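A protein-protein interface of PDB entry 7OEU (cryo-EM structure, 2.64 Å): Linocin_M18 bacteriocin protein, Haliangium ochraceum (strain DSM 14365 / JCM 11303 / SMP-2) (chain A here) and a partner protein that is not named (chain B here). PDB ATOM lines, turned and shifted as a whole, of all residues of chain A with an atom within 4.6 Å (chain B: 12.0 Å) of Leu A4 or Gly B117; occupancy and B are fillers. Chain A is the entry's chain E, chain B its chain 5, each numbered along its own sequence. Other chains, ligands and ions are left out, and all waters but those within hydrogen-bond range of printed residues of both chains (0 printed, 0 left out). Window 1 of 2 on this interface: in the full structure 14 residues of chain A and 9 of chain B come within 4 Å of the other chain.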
ATOM      1  N   ASP A   2     -15.376  14.064   9.848  1.00  0.00           N
ATOM      2  CA  ASP A   2     -14.615  13.725  11.038  1.00  0.00           C
ATOM      3  C   ASP A   2     -13.569  14.808  11.307  1.00  0.00           C
ATOM      4  O   ASP A   2     -13.570  15.873  10.685  1.00  0.00           O
ATOM      5  CB  ASP A   2     -14.003  12.334  10.886  1.00  0.00           C
ATOM      6  CG  ASP A   2     -12.886  12.283   9.852  1.00  0.00           C
ATOM      7  OD1 ASP A   2     -12.164  11.267   9.821  1.00  0.00           O
ATOM      8  OD2 ASP A   2     -12.736  13.235   9.060  1.00  0.00           O
ATOM      9  N   LEU A   3     -12.660  14.540  12.242  1.00  0.00           N
ATOM     10  CA  LEU A   3     -11.632  15.511  12.595  1.00  0.00           C
ATOM     11  C   LEU A   3     -10.620  15.742  11.478  1.00  0.00           C
ATOM     12  O   LEU A   3      -9.912  16.751  11.509  1.00  0.00           O
ATOM     13  CB  LEU A   3     -10.907  15.061  13.861  1.00  0.00           C
ATOM     14  CG  LEU A   3     -11.604  15.387  15.177  1.00  0.00           C
ATOM     15  CD1 LEU A   3     -10.915  14.685  16.329  1.00  0.00           C
ATOM     16  CD2 LEU A   3     -11.634  16.886  15.399  1.00  0.00           C
ATOM     17  N   LEU A   4     -10.530  14.840  10.501  1.00  0.00           N
ATOM     18  CA  LEU A   4      -9.570  15.027   9.421  1.00  0.00           C
ATOM     19  C   LEU A   4     -10.029  16.077   8.417  1.00  0.00           C
ATOM     20  O   LEU A   4      -9.190  16.693   7.755  1.00  0.00           O
ATOM     21  CB  LEU A   4      -9.293  13.695   8.727  1.00  0.00           C
ATOM     22  CG  LEU A   4      -8.747  12.602   9.652  1.00  0.00           C
ATOM     23  CD1 LEU A   4      -8.645  11.272   8.934  1.00  0.00           C
ATOM     24  CD2 LEU A   4      -7.403  13.002  10.240  1.00  0.00           C
ATOM     25  N   LYS A   5     -11.341  16.295   8.295  1.00  0.00           N
ATOM     26  CA  LYS A   5     -11.903  17.403   7.516  1.00  0.00           C
ATOM     27  C   LYS A   5     -11.436  17.371   6.063  1.00  0.00           C
ATOM     28  O   LYS A   5     -11.165  18.409   5.459  1.00  0.00           O
ATOM     29  CB  LYS A   5     -11.557  18.751   8.151  1.00  0.00           C
ATOM     30  CG  LYS A   5     -11.906  18.873   9.616  1.00  0.00           C
ATOM     31  CD  LYS A   5     -11.635  20.277  10.113  1.00  0.00           C
ATOM     32  CE  LYS A   5     -11.921  20.415  11.599  1.00  0.00           C
ATOM     33  NZ  LYS A   5     -13.231  19.821  11.965  1.00  0.00           N
ATOM     34  N   ARG A   6     -11.346  16.171   5.492  1.00  0.00           N
ATOM     35  CA  ARG A   6     -10.715  16.032   4.184  1.00  0.00           C
ATOM     36  C   ARG A   6     -11.588  16.583   3.063  1.00  0.00           C
ATOM     37  O   ARG A   6     -11.062  17.023   2.035  1.00  0.00           O
ATOM     38  CB  ARG A   6     -10.370  14.571   3.924  1.00  0.00           C
ATOM     39  CG  ARG A   6      -9.049  14.159   4.539  1.00  0.00           C
ATOM     40  CD  ARG A   6      -8.980  12.676   4.756  1.00  0.00           C
ATOM     41  NE  ARG A   6      -8.754  11.960   3.509  1.00  0.00           N
ATOM     42  CZ  ARG A   6      -7.666  11.247   3.248  1.00  0.00           C
ATOM     43  NH1 ARG A   6      -6.696  11.164   4.145  1.00  0.00           N
ATOM     44  NH2 ARG A   6      -7.546  10.623   2.089  1.00  0.00           N
ATOM     45  N   TRP A  45     -10.814   8.177  18.058  1.00  0.00           N
ATOM     46  CA  TRP A  45     -10.460   9.496  18.565  1.00  0.00           C
ATOM     47  C   TRP A  45     -10.825   9.712  20.027  1.00  0.00           C
ATOM     48  O   TRP A  45     -10.267  10.614  20.658  1.00  0.00           O
ATOM     49  CB  TRP A  45     -11.143  10.578  17.730  1.00  0.00           C
ATOM     50  CG  TRP A  45     -10.588  10.770  16.360  1.00  0.00           C
ATOM     51  CD1 TRP A  45     -11.139  10.351  15.191  1.00  0.00           C
ATOM     52  CD2 TRP A  45      -9.389  11.468  16.011  1.00  0.00           C
ATOM     53  NE1 TRP A  45     -10.353  10.727  14.135  1.00  0.00           N
ATOM     54  CE2 TRP A  45      -9.272  11.419  14.612  1.00  0.00           C
ATOM     55  CE3 TRP A  45      -8.400  12.123  16.747  1.00  0.00           C
ATOM     56  CZ2 TRP A  45      -8.209  11.996  13.934  1.00  0.00           C
ATOM     57  CZ3 TRP A  45      -7.346  12.696  16.072  1.00  0.00           C
ATOM     58  CH2 TRP A  45      -7.257  12.629  14.680  1.00  0.00           C
ATOM     59  N   SER A 231      -3.094   8.864  10.253  1.00  0.00           N
ATOM     60  CA  SER A 231      -4.090   9.425   9.354  1.00  0.00           C
ATOM     61  C   SER A 231      -3.546  10.699   8.729  1.00  0.00           C
ATOM     62  O   SER A 231      -2.677  11.366   9.289  1.00  0.00           O
ATOM     63  CB  SER A 231      -5.401   9.732  10.086  1.00  0.00           C
ATOM     64  OG  SER A 231      -5.852   8.614  10.820  1.00  0.00           O
ATOM     65  N   ILE A 232      -4.079  11.037   7.562  1.00  0.00           N
ATOM     66  CA  ILE A 232      -3.771  12.290   6.888  1.00  0.00           C
ATOM     67  C   ILE A 232      -5.004  13.175   6.963  1.00  0.00           C
ATOM     68  O   ILE A 232      -6.081  12.796   6.489  1.00  0.00           O
ATOM     69  CB  ILE A 232      -3.336  12.071   5.431  1.00  0.00           C
ATOM     70  CG1 ILE A 232      -2.228  11.021   5.353  1.00  0.00           C
ATOM     71  CG2 ILE A 232      -2.894  13.383   4.815  1.00  0.00           C
ATOM     72  CD1 ILE A 232      -0.905  11.488   5.896  1.00  0.00           C
ATOM     73  N   GLY A 233      -4.848  14.355   7.565  1.00  0.00           N
ATOM     74  CA  GLY A 233      -5.925  15.304   7.695  1.00  0.00           C
ATOM     75  C   GLY A 233      -5.590  16.626   7.021  1.00  0.00           C
ATOM     76  O   GLY A 233      -4.437  16.918   6.704  1.00  0.00           O
ATOM     77  N   TYR A 234      -6.629  17.425   6.817  1.00  0.00           N
ATOM     78  CA  TYR A 234      -6.513  18.736   6.198  1.00  0.00           C
ATOM     79  C   TYR A 234      -6.615  19.817   7.263  1.00  0.00           C
ATOM     80  O   TYR A 234      -7.467  19.744   8.150  1.00  0.00           O
ATOM     81  CB  TYR A 234      -7.603  18.924   5.141  1.00  0.00           C
ATOM     82  CG  TYR A 234      -7.858  20.362   4.763  1.00  0.00           C
ATOM     83  CD1 TYR A 234      -7.005  21.037   3.906  1.00  0.00           C
ATOM     84  CD2 TYR A 234      -8.954  21.047   5.268  1.00  0.00           C
ATOM     85  CE1 TYR A 234      -7.234  22.342   3.559  1.00  0.00           C
ATOM     86  CE2 TYR A 234      -9.188  22.358   4.930  1.00  0.00           C
ATOM     87  CZ  TYR A 234      -8.328  23.001   4.074  1.00  0.00           C
ATOM     88  OH  TYR A 234      -8.559  24.309   3.734  1.00  0.00           O
ATOM     89  N   PHE A 245      -1.700  17.356   7.525  1.00  0.00           N
ATOM     90  CA  PHE A 245      -0.954  16.860   8.667  1.00  0.00           C
ATOM     91  C   PHE A 245      -1.073  15.350   8.735  1.00  0.00           C
ATOM     92  O   PHE A 245      -2.038  14.761   8.244  1.00  0.00           O
ATOM     93  CB  PHE A 245      -1.429  17.488   9.986  1.00  0.00           C
ATOM     94  CG  PHE A 245      -2.894  17.299  10.260  1.00  0.00           C
ATOM     95  CD1 PHE A 245      -3.816  18.251   9.859  1.00  0.00           C
ATOM     96  CD2 PHE A 245      -3.352  16.168  10.916  1.00  0.00           C
ATOM     97  CE1 PHE A 245      -5.159  18.081  10.107  1.00  0.00           C
ATOM     98  CE2 PHE A 245      -4.695  15.992  11.165  1.00  0.00           C
ATOM     99  CZ  PHE A 245      -5.600  16.951  10.760  1.00  0.00           C
ATOM    100  N   GLY B 117     -10.972   6.720   9.561  1.00  0.00           N
ATOM    101  CA  GLY B 117     -10.422   7.051   8.259  1.00  0.00           C
ATOM    102  C   GLY B 117      -8.912   7.185   8.258  1.00  0.00           C
ATOM    103  O   GLY B 117      -8.366   8.159   7.749  1.00  0.00           O
ATOM    104  N   SER B 118      -8.235   6.196   8.828  1.00  0.00           N
ATOM    105  CA  SER B 118      -6.787   6.211   8.929  1.00  0.00           C
ATOM    106  C   SER B 118      -6.158   5.625   7.667  1.00  0.00           C
ATOM    107  O   SER B 118      -6.843   5.200   6.736  1.00  0.00           O
ATOM    108  CB  SER B 118      -6.337   5.447  10.172  1.00  0.00           C
ATOM    109  OG  SER B 118      -6.453   4.052   9.973  1.00  0.00           O
ATOM    110  N   LEU B 119      -4.826   5.604   7.639  1.00  0.00           N
ATOM    111  CA  LEU B 119      -4.097   4.981   6.542  1.00  0.00           C
ATOM    112  C   LEU B 119      -4.100   3.463   6.624  1.00  0.00           C
ATOM    113  O   LEU B 119      -3.640   2.809   5.683  1.00  0.00           O
ATOM    114  CB  LEU B 119      -2.660   5.498   6.510  1.00  0.00           C
ATOM    115  CG  LEU B 119      -2.514   7.013   6.355  1.00  0.00           C
ATOM    116  CD1 LEU B 119      -1.167   7.481   6.868  1.00  0.00           C
ATOM    117  CD2 LEU B 119      -2.720   7.423   4.907  1.00  0.00           C
ATOM    118  N   GLY B 120      -4.605   2.892   7.711  1.00  0.00           N
ATOM    119  CA  GLY B 120      -4.665   1.449   7.862  1.00  0.00           C
ATOM    120  C   GLY B 120      -3.323   0.767   8.017  1.00  0.00           C
ATOM    121  O   GLY B 120      -3.111  -0.306   7.440  1.00  0.00           O
ATOM    122  N   ILE B 121      -2.411   1.359   8.782  1.00  0.00           N
ATOM    123  CA  ILE B 121      -1.122   0.721   9.031  1.00  0.00           C
ATOM    124  C   ILE B 121      -1.274  -0.420  10.028  1.00  0.00           C
ATOM    125  O   ILE B 121      -0.970  -1.579   9.723  1.00  0.00           O
ATOM    126  CB  ILE B 121      -0.088   1.753   9.518  1.00  0.00           C
ATOM    127  CG1 ILE B 121       0.041   2.913   8.526  1.00  0.00           C
ATOM    128  CG2 ILE B 121       1.258   1.082   9.749  1.00  0.00           C
ATOM    129  CD1 ILE B 121       0.075   2.493   7.073  1.00  0.00           C
ATOM    130  N   GLY B 122      -1.747  -0.107  11.233  1.00  0.00           N
ATOM    131  CA  GLY B 122      -1.944  -1.125  12.243  1.00  0.00           C
ATOM    132  C   GLY B 122      -0.631  -1.731  12.709  1.00  0.00           C
ATOM    133  O   GLY B 122       0.433  -1.105  12.667  1.00  0.00           O
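The backbone NH of Leu A4 sits at hydrogen-bond distance from the side-chain carboxylate of Asp A2 (3.1 Å). NH1 of Arg A6 sits at hydrogen-bond distance from O of Ile A232. The backbone carbonyl oxygen of Leu A4 is in hydrogen-bond range of the backbone NH of Tyr A234. The side-chain hydroxyl (OG) of Ser B118 sits at hydrogen-bond distance from the backbone NH (N) of Gly B120 (3.1 Å).
Among the printed residues, pairs that only touch across the chains: Leu A4 with Gly B117, Ser A231 with Gly B117, Ser A231 with Ser B118 and Ile A232 with Leu B119.
Of chain B, only Gly B117 (3.3 Å) comes within 4 Å of Leu A4. Of the printed residues of chain A, Gly B117 touches Leu A4 (3.3 Å) and Ser A231 (3.99 Å). No residue of chain B comes within 4 Å of Lys A5. No residue of chain B comes within 4 Å of Phe A245. Of the printed residues of chain B, Ile A232 touches Leu B119 (3.7 Å). Printed residues of chain A within 4 Å of Ser B118: Ser A231. The nearest residue of chain B that does not touch Leu A4 is Ser B118 (5.1 Å). The nearest printed residue of chain A that does not touch Gly B117 is Asp A2 (4.7 Å).
Of the 6 printed residues of chain B, 3 touch a printed residue of chain A. Hydrophobic or aromatic side chains of chain B within 4 Å of the printed part of chain A: Leu B119. Hydrophobic or aromatic side chains of chain A within 4 Å of the printed part of chain B: Leu A4 and Ile A232. Along chain A the printed residues that touch a printed residue of chain B span positions 4 to 232. Among the printed residues, 4 pairs touch across the chains.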
